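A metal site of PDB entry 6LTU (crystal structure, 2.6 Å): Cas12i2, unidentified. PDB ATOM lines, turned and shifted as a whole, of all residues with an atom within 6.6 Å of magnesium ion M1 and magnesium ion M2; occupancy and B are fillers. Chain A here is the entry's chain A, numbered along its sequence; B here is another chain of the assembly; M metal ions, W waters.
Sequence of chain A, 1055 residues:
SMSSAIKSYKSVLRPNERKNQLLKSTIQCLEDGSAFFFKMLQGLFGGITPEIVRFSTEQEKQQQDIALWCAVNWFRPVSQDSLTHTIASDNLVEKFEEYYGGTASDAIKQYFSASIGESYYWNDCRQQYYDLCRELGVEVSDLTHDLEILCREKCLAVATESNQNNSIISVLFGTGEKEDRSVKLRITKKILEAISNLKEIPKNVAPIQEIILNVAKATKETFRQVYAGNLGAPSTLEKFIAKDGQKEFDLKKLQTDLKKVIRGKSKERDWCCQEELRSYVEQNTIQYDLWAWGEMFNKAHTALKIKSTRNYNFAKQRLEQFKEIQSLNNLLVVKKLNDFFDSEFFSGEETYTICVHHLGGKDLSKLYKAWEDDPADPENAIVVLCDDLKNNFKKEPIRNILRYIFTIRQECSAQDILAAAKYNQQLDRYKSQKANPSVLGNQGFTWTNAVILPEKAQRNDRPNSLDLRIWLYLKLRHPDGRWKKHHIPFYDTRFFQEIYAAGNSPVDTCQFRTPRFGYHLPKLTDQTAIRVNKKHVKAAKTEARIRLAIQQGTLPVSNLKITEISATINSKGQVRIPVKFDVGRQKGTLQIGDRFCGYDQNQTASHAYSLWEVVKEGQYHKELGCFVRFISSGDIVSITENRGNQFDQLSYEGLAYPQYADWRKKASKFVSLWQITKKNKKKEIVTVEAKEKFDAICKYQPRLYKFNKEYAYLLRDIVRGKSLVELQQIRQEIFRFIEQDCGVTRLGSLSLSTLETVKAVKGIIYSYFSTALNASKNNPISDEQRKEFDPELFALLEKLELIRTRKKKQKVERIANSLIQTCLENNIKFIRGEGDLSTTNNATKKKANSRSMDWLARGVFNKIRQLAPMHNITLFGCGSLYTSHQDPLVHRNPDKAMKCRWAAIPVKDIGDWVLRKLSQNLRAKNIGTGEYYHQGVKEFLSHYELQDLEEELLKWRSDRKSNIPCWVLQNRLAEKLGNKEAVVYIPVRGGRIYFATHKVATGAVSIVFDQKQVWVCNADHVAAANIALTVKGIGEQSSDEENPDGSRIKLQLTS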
ATOM      1  N   TYR A 599      31.152  19.829 -19.867  1.00  0.00           N
ATOM      2  CA  TYR A 599      32.097  19.401 -18.852  1.00  0.00           C
ATOM      3  C   TYR A 599      31.387  19.027 -17.550  1.00  0.00           C
ATOM      4  O   TYR A 599      30.443  19.693 -17.126  1.00  0.00           O
ATOM      5  CB  TYR A 599      33.182  20.454 -18.598  1.00  0.00           C
ATOM      6  CG  TYR A 599      32.745  21.673 -17.831  1.00  0.00           C
ATOM      7  CD1 TYR A 599      32.901  21.736 -16.448  1.00  0.00           C
ATOM      8  CD2 TYR A 599      32.191  22.757 -18.483  1.00  0.00           C
ATOM      9  CE1 TYR A 599      32.505  22.859 -15.745  1.00  0.00           C
ATOM     10  CE2 TYR A 599      31.789  23.883 -17.787  1.00  0.00           C
ATOM     11  CZ  TYR A 599      31.948  23.928 -16.416  1.00  0.00           C
ATOM     12  OH  TYR A 599      31.538  25.048 -15.730  1.00  0.00           O
ATOM     13  N   ASP A 600      31.865  17.949 -16.942  1.00  0.00           N
ATOM     14  CA  ASP A 600      31.367  17.409 -15.688  1.00  0.00           C
ATOM     15  C   ASP A 600      32.380  17.681 -14.583  1.00  0.00           C
ATOM     16  O   ASP A 600      33.558  17.332 -14.718  1.00  0.00           O
ATOM     17  CB  ASP A 600      31.105  15.908 -15.804  1.00  0.00           C
ATOM     18  CG  ASP A 600      30.878  15.237 -14.465  1.00  0.00           C
ATOM     19  OD1 ASP A 600      29.991  15.682 -13.702  1.00  0.00           O
ATOM     20  OD2 ASP A 600      31.599  14.266 -14.155  1.00  0.00           O
ATOM     21  N   GLN A 601      31.909  18.290 -13.491  1.00  0.00           N
ATOM     22  CA  GLN A 601      32.757  18.642 -12.362  1.00  0.00           C
ATOM     23  C   GLN A 601      32.752  17.515 -11.335  1.00  0.00           C
ATOM     24  O   GLN A 601      31.694  17.143 -10.819  1.00  0.00           O
ATOM     25  CB  GLN A 601      32.279  19.942 -11.704  1.00  0.00           C
ATOM     26  CG  GLN A 601      32.480  21.188 -12.540  1.00  0.00           C
ATOM     27  CD  GLN A 601      32.737  22.421 -11.679  1.00  0.00           C
ATOM     28  OE1 GLN A 601      33.688  22.459 -10.904  1.00  0.00           O
ATOM     29  NE2 GLN A 601      31.877  23.428 -11.826  1.00  0.00           N
ATOM     30  N   ASN A 602      33.932  16.983 -11.039  1.00  0.00           N
ATOM     31  CA  ASN A 602      34.104  15.925 -10.048  1.00  0.00           C
ATOM     32  C   ASN A 602      34.935  16.441  -8.887  1.00  0.00           C
ATOM     33  O   ASN A 602      35.588  17.485  -8.977  1.00  0.00           O
ATOM     34  CB  ASN A 602      34.755  14.690 -10.686  1.00  0.00           C
ATOM     35  CG  ASN A 602      33.940  14.149 -11.844  1.00  0.00           C
ATOM     36  OD1 ASN A 602      32.821  13.682 -11.667  1.00  0.00           O
ATOM     37  ND2 ASN A 602      34.507  14.218 -13.048  1.00  0.00           N
ATOM     38  N   SER A 606      39.054  13.529 -11.893  1.00  0.00           N
ATOM     39  CA  SER A 606      39.224  14.693 -12.753  1.00  0.00           C
ATOM     40  C   SER A 606      37.890  15.137 -13.345  1.00  0.00           C
ATOM     41  O   SER A 606      37.012  14.328 -13.639  1.00  0.00           O
ATOM     42  CB  SER A 606      40.207  14.393 -13.880  1.00  0.00           C
ATOM     43  OG  SER A 606      41.471  14.007 -13.369  1.00  0.00           O
ATOM     44  N   GLU A 834      27.367  22.547 -15.788  1.00  0.00           N
ATOM     45  CA  GLU A 834      26.389  22.554 -14.713  1.00  0.00           C
ATOM     46  C   GLU A 834      26.438  23.898 -13.986  1.00  0.00           C
ATOM     47  O   GLU A 834      27.433  24.210 -13.320  1.00  0.00           O
ATOM     48  CB  GLU A 834      26.654  21.425 -13.723  1.00  0.00           C
ATOM     49  CG  GLU A 834      26.654  20.033 -14.347  1.00  0.00           C
ATOM     50  CD  GLU A 834      27.578  19.071 -13.608  1.00  0.00           C
ATOM     51  OE1 GLU A 834      28.795  19.354 -13.535  1.00  0.00           O
ATOM     52  OE2 GLU A 834      27.093  18.031 -13.118  1.00  0.00           O
ATOM     53  N   LEU A 837      25.214  23.445  -9.335  1.00  0.00           N
ATOM     54  CA  LEU A 837      25.783  22.591  -8.300  1.00  0.00           C
ATOM     55  C   LEU A 837      25.606  23.193  -6.905  1.00  0.00           C
ATOM     56  O   LEU A 837      25.613  24.407  -6.715  1.00  0.00           O
ATOM     57  CB  LEU A 837      27.259  22.340  -8.590  1.00  0.00           C
ATOM     58  CG  LEU A 837      27.419  21.782 -10.020  1.00  0.00           C
ATOM     59  CD1 LEU A 837      28.855  21.861 -10.516  1.00  0.00           C
ATOM     60  CD2 LEU A 837      26.889  20.356 -10.094  1.00  0.00           C
ATOM     61  N   TRP A 855      35.541  22.505  -2.766  1.00  0.00           N
ATOM     62  CA  TRP A 855      35.346  21.998  -4.119  1.00  0.00           C
ATOM     63  C   TRP A 855      35.334  23.119  -5.150  1.00  0.00           C
ATOM     64  O   TRP A 855      35.920  22.971  -6.231  1.00  0.00           O
ATOM     65  CB  TRP A 855      34.038  21.201  -4.179  1.00  0.00           C
ATOM     66  CG  TRP A 855      33.812  20.471  -5.467  1.00  0.00           C
ATOM     67  CD1 TRP A 855      34.770  19.994  -6.319  1.00  0.00           C
ATOM     68  CD2 TRP A 855      32.551  20.124  -6.046  1.00  0.00           C
ATOM     69  NE1 TRP A 855      34.172  19.375  -7.392  1.00  0.00           N
ATOM     70  CE2 TRP A 855      32.810  19.443  -7.253  1.00  0.00           C
ATOM     71  CE3 TRP A 855      31.220  20.331  -5.663  1.00  0.00           C
ATOM     72  CZ2 TRP A 855      31.793  18.956  -8.075  1.00  0.00           C
ATOM     73  CZ3 TRP A 855      30.211  19.850  -6.475  1.00  0.00           C
ATOM     74  CH2 TRP A 855      30.505  19.169  -7.672  1.00  0.00           C
ATOM     75  N   SER A 880      22.041  20.396 -13.507  1.00  0.00           N
ATOM     76  CA  SER A 880      22.861  19.211 -13.336  1.00  0.00           C
ATOM     77  C   SER A 880      22.058  17.943 -13.093  1.00  0.00           C
ATOM     78  O   SER A 880      22.626  16.848 -13.139  1.00  0.00           O
ATOM     79  CB  SER A 880      23.848  19.410 -12.172  1.00  0.00           C
ATOM     80  OG  SER A 880      23.166  19.354 -10.934  1.00  0.00           O
ATOM     81  N   THR A 883      22.190  14.269 -15.006  1.00  0.00           N
ATOM     82  CA  THR A 883      23.214  14.252 -16.042  1.00  0.00           C
ATOM     83  C   THR A 883      24.220  13.123 -15.865  1.00  0.00           C
ATOM     84  O   THR A 883      24.980  12.848 -16.805  1.00  0.00           O
ATOM     85  CB  THR A 883      23.950  15.594 -16.083  1.00  0.00           C
ATOM     86  OG1 THR A 883      24.506  15.876 -14.792  1.00  0.00           O
ATOM     87  CG2 THR A 883      23.006  16.713 -16.498  1.00  0.00           C
ATOM     88  N   SER A 884      24.262  12.477 -14.704  1.00  0.00           N
ATOM     89  CA  SER A 884      25.157  11.349 -14.487  1.00  0.00           C
ATOM     90  C   SER A 884      24.530  10.010 -14.844  1.00  0.00           C
ATOM     91  O   SER A 884      25.226   8.990 -14.798  1.00  0.00           O
ATOM     92  CB  SER A 884      25.614  11.320 -13.029  1.00  0.00           C
ATOM     93  OG  SER A 884      26.407  12.447 -12.715  1.00  0.00           O
ATOM     94  N   ARG A 901      24.935   3.483 -12.432  1.00  0.00           N
ATOM     95  CA  ARG A 901      26.367   3.559 -12.608  1.00  0.00           C
ATOM     96  C   ARG A 901      27.020   2.318 -11.999  1.00  0.00           C
ATOM     97  O   ARG A 901      26.474   1.702 -11.086  1.00  0.00           O
ATOM     98  CB  ARG A 901      26.942   4.832 -11.973  1.00  0.00           C
ATOM     99  CG  ARG A 901      26.571   6.103 -12.711  1.00  0.00           C
ATOM    100  CD  ARG A 901      26.724   7.331 -11.833  1.00  0.00           C
ATOM    101  NE  ARG A 901      28.131   7.681 -11.641  1.00  0.00           N
ATOM    102  CZ  ARG A 901      28.551   8.838 -11.163  1.00  0.00           C
ATOM    103  NH1 ARG A 901      27.678   9.775 -10.816  1.00  0.00           N
ATOM    104  NH2 ARG A 901      29.854   9.063 -11.021  1.00  0.00           N
ATOM    105  N   ARG A 992      32.423   4.731 -11.491  1.00  0.00           N
ATOM    106  CA  ARG A 992      33.112   5.385 -12.606  1.00  0.00           C
ATOM    107  C   ARG A 992      32.875   4.690 -13.938  1.00  0.00           C
ATOM    108  O   ARG A 992      33.557   5.013 -14.918  1.00  0.00           O
ATOM    109  CB  ARG A 992      34.619   5.456 -12.320  1.00  0.00           C
ATOM    110  CG  ARG A 992      34.981   6.153 -11.011  1.00  0.00           C
ATOM    111  CD  ARG A 992      34.730   7.647 -11.071  1.00  0.00           C
ATOM    112  NE  ARG A 992      35.121   8.326  -9.836  1.00  0.00           N
ATOM    113  CZ  ARG A 992      34.671   9.518  -9.459  1.00  0.00           C
ATOM    114  NH1 ARG A 992      33.807  10.186 -10.214  1.00  0.00           N
ATOM    115  NH2 ARG A 992      35.094  10.048  -8.317  1.00  0.00           N
ATOM    116  N   ALA A1019      32.230   6.903 -16.662  1.00  0.00           N
ATOM    117  CA  ALA A1019      30.949   7.476 -16.269  1.00  0.00           C
ATOM    118  C   ALA A1019      30.980   8.999 -16.334  1.00  0.00           C
ATOM    119  O   ALA A1019      29.986   9.633 -16.716  1.00  0.00           O
ATOM    120  CB  ALA A1019      30.571   7.026 -14.855  1.00  0.00           C
ATOM    121  N   ASP A1020      32.108   9.614 -15.981  1.00  0.00           N
ATOM    122  CA  ASP A1020      32.182  11.071 -16.030  1.00  0.00           C
ATOM    123  C   ASP A1020      32.241  11.581 -17.464  1.00  0.00           C
ATOM    124  O   ASP A1020      31.739  12.668 -17.743  1.00  0.00           O
ATOM    125  CB  ASP A1020      33.383  11.567 -15.222  1.00  0.00           C
ATOM    126  CG  ASP A1020      33.306  11.148 -13.759  1.00  0.00           C
ATOM    127  OD1 ASP A1020      32.273  11.426 -13.127  1.00  0.00           O
ATOM    128  OD2 ASP A1020      34.279  10.550 -13.261  1.00  0.00           O
ATOM    129  N   ALA A1023      28.752  11.671 -18.375  1.00  0.00           N
ATOM    130  CA  ALA A1023      28.113  12.844 -17.789  1.00  0.00           C
ATOM    131  C   ALA A1023      28.429  14.097 -18.581  1.00  0.00           C
ATOM    132  O   ALA A1023      27.560  14.945 -18.792  1.00  0.00           O
ATOM    133  CB  ALA A1023      28.538  13.001 -16.331  1.00  0.00           C
ATOM    134  N   ILE A1027      25.800  16.574 -20.422  1.00  0.00           N
ATOM    135  CA  ILE A1027      25.792  18.016 -20.241  1.00  0.00           C
ATOM    136  C   ILE A1027      25.897  18.724 -21.583  1.00  0.00           C
ATOM    137  O   ILE A1027      25.191  19.710 -21.844  1.00  0.00           O
ATOM    138  CB  ILE A1027      26.925  18.432 -19.285  1.00  0.00           C
ATOM    139  CG1 ILE A1027      26.579  18.042 -17.845  1.00  0.00           C
ATOM    140  CG2 ILE A1027      27.204  19.924 -19.382  1.00  0.00           C
ATOM    141  CD1 ILE A1027      27.783  17.730 -16.984  1.00  0.00           C
ATOM    142  P    DC B   2      22.328  12.523 -10.724  1.00  0.00           P
ATOM    143  OP1  DC B   2      22.335  11.770 -11.985  1.00  0.00           O
ATOM    144  OP2  DC B   2      22.627  11.850  -9.460  1.00  0.00           O
ATOM    145  O5'  DC B   2      23.340  13.720 -10.940  1.00  0.00           O
ATOM    146  C5'  DC B   2      24.231  14.052  -9.885  1.00  0.00           C
ATOM    147  C4'  DC B   2      24.987  15.311 -10.216  1.00  0.00           C
ATOM    148  O4'  DC B   2      24.208  16.398  -9.675  1.00  0.00           O
ATOM    149  C3'  DC B   2      26.329  15.336  -9.490  1.00  0.00           C
ATOM    150  O3'  DC B   2      27.386  15.166 -10.415  1.00  0.00           O
ATOM    151  C2'  DC B   2      26.381  16.687  -8.791  1.00  0.00           C
ATOM    152  C1'  DC B   2      24.974  17.258  -8.874  1.00  0.00           C
ATOM    153  N1   DC B   2      24.341  17.310  -7.559  1.00  0.00           N
ATOM    154  C2   DC B   2      24.438  18.485  -6.796  1.00  0.00           C
ATOM    155  O2   DC B   2      25.063  19.439  -7.263  1.00  0.00           O
ATOM    156  N3   DC B   2      23.847  18.536  -5.586  1.00  0.00           N
ATOM    157  C4   DC B   2      23.178  17.478  -5.128  1.00  0.00           C
ATOM    158  N4   DC B   2      22.611  17.576  -3.918  1.00  0.00           N
ATOM    159  C5   DC B   2      23.060  16.279  -5.870  1.00  0.00           C
ATOM    160  C6   DC B   2      23.646  16.238  -7.070  1.00  0.00           C
ATOM    161  P    DC B   3      28.242  13.853 -10.345  1.00  0.00           P
ATOM    162  OP1  DC B   3      29.194  13.878 -11.481  1.00  0.00           O
ATOM    163  OP2  DC B   3      27.332  12.706 -10.193  1.00  0.00           O
ATOM    164  O5'  DC B   3      29.049  14.042  -8.976  1.00  0.00           O
ATOM    165  C5'  DC B   3      29.795  15.233  -8.746  1.00  0.00           C
ATOM    166  C4'  DC B   3      30.053  15.429  -7.267  1.00  0.00           C
ATOM    167  O4'  DC B   3      28.844  15.830  -6.609  1.00  0.00           O
ATOM    168  C3'  DC B   3      30.480  14.176  -6.525  1.00  0.00           C
ATOM    169  O3'  DC B   3      31.894  14.029  -6.605  1.00  0.00           O
ATOM    170  C2'  DC B   3      30.023  14.443  -5.085  1.00  0.00           C
ATOM    171  C1'  DC B   3      28.957  15.533  -5.227  1.00  0.00           C
ATOM    172  N1   DC B   3      27.618  15.135  -4.719  1.00  0.00           N
ATOM    173  C2   DC B   3      27.015  15.885  -3.701  1.00  0.00           C
ATOM    174  O2   DC B   3      27.610  16.868  -3.254  1.00  0.00           O
ATOM    175  N3   DC B   3      25.798  15.506  -3.234  1.00  0.00           N
ATOM    176  C4   DC B   3      25.192  14.427  -3.742  1.00  0.00           C
ATOM    177  N4   DC B   3      23.991  14.092  -3.255  1.00  0.00           N
ATOM    178  C5   DC B   3      25.791  13.652  -4.782  1.00  0.00           C
ATOM    179  C6   DC B   3      26.995  14.040  -5.234  1.00  0.00           C
ATOM    180  P    DT B   4      32.533  12.608  -6.982  1.00  0.00           P
ATOM    181  OP1  DT B   4      33.974  12.828  -7.267  1.00  0.00           O
ATOM    182  OP2  DT B   4      31.659  11.991  -8.013  1.00  0.00           O
ATOM    183  O5'  DT B   4      32.387  11.742  -5.648  1.00  0.00           O
ATOM    184  C5'  DT B   4      33.191  12.027  -4.512  1.00  0.00           C
ATOM    185  C4'  DT B   4      32.999  10.984  -3.425  1.00  0.00           C
ATOM    186  O4'  DT B   4      31.591  10.850  -3.130  1.00  0.00           O
ATOM    187  C3'  DT B   4      33.511   9.584  -3.782  1.00  0.00           C
ATOM    188  O3'  DT B   4      34.281   9.060  -2.715  1.00  0.00           O
ATOM    189  C2'  DT B   4      32.240   8.775  -4.017  1.00  0.00           C
ATOM    190  C1'  DT B   4      31.216   9.485  -3.157  1.00  0.00           C
ATOM    191  N1   DT B   4      29.831   9.409  -3.703  1.00  0.00           N
ATOM    192  C2   DT B   4      28.842   8.812  -2.958  1.00  0.00           C
ATOM    193  O2   DT B   4      29.031   8.331  -1.849  1.00  0.00           O
ATOM    194  N3   DT B   4      27.609   8.792  -3.554  1.00  0.00           N
ATOM    195  C4   DT B   4      27.274   9.300  -4.804  1.00  0.00           C
ATOM    196  O4   DT B   4      26.140   9.240  -5.252  1.00  0.00           O
ATOM    197  C5   DT B   4      28.360   9.913  -5.527  1.00  0.00           C
ATOM    198  C7   DT B   4      28.128  10.503  -6.885  1.00  0.00           C
ATOM    199  C6   DT B   4      29.580   9.939  -4.946  1.00  0.00           C
HETATM  200 MG    MG M   1      30.812  13.192 -12.518  1.00  0.00          MG
HETATM  201 MG    MG M   2      28.175  16.113 -12.707  1.00  0.00          MG
HETATM  202  O   HOH W   1      29.180  11.957 -13.165  1.00  0.00           O
HETATM  203  O   HOH W   2      29.406  17.724 -11.327  1.00  0.00           O
HETATM  204  O   HOH W   3      31.239  11.814 -10.708  1.00  0.00           O
HETATM  205  O   HOH W   4      26.908  14.746 -13.794  1.00  0.00           O
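O4' of DC 2 of chain B is in hydrogen-bond range of the side-chain hydroxyl of Ser 880.
The side-chain carboxylate (OD1) of Asp 1020 lies close to the guanidinium group (NH2) of Arg 901 (3.98 Å).
OP1 of DC 2 of chain B is in hydrogen-bond range of the backbone NH of Ser 884, at 3.4 Å.
ND2 of Asn 602 is in hydrogen-bond range of O of Ser 606, 2.6 Å away.
OP2 of DC 3 of chain B lies within salt-bridge range of NH1 of Arg 901 (3.0 Å).
OP2 of DC 3 of chain B lies within hydrogen-bond range of the side-chain hydroxyl (OG) of Ser 884, at 2.7 Å.
The side-chain carboxylate (OD2) of Asp 1020 is in salt-bridge range of the guanidinium group (NH1) of Arg 992, 3.1 Å away.
The side-chain carboxylate (OE1) of Glu 834 is in hydrogen-bond range of the backbone NH (N) of Gln 601 (3.3 Å).
Within 4 Å of magnesium ion M1: Asp 600, Asn 602, Asp 1020 and DC 3 of chain B.
Of the 20 residues printed, 4 come within 4 Å of magnesium ion M2.
The nearest printed residue that does not touch magnesium ion M2 is Ser 884 (4.1 Å).
Magnesium ion M1 is bound by OP1 of DC 3 of chain B (2.0 Å), OD2 of Asp 600 (2.1 Å), water W1 (2.1 Å), OD1 of Asn 602 (2.2 Å), water W3 (2.3 Å) and OD1 of Asp 1020 (2.4 Å).
Magnesium ion M1 has six donor atoms within binding distance.
Magnesium ion M2 is bound by OD1 of Asp 600 (2.1 Å), water W4 (2.2 Å), OE2 of Glu 834 (2.2 Å) and water W2 (2.5 Å).
Slightly farther from magnesium ion M2 lies O3' of DC 2 of chain B (2.6 Å).
Slightly farther from magnesium ion M2 lies OP1 of DC 3 of chain B (2.7 Å).
Water W3 lies within hydrogen-bond range of OP2 of DT 4 of chain B (2.7 Å), the guanidinium group of Arg 992 (3.1 Å) and the guanidinium group of Arg 901 (3.1 Å).
Water W4 lies within hydrogen-bond range of OG of Ser 884, OG1 of Thr 883 and O3' of DC 2 of chain B.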
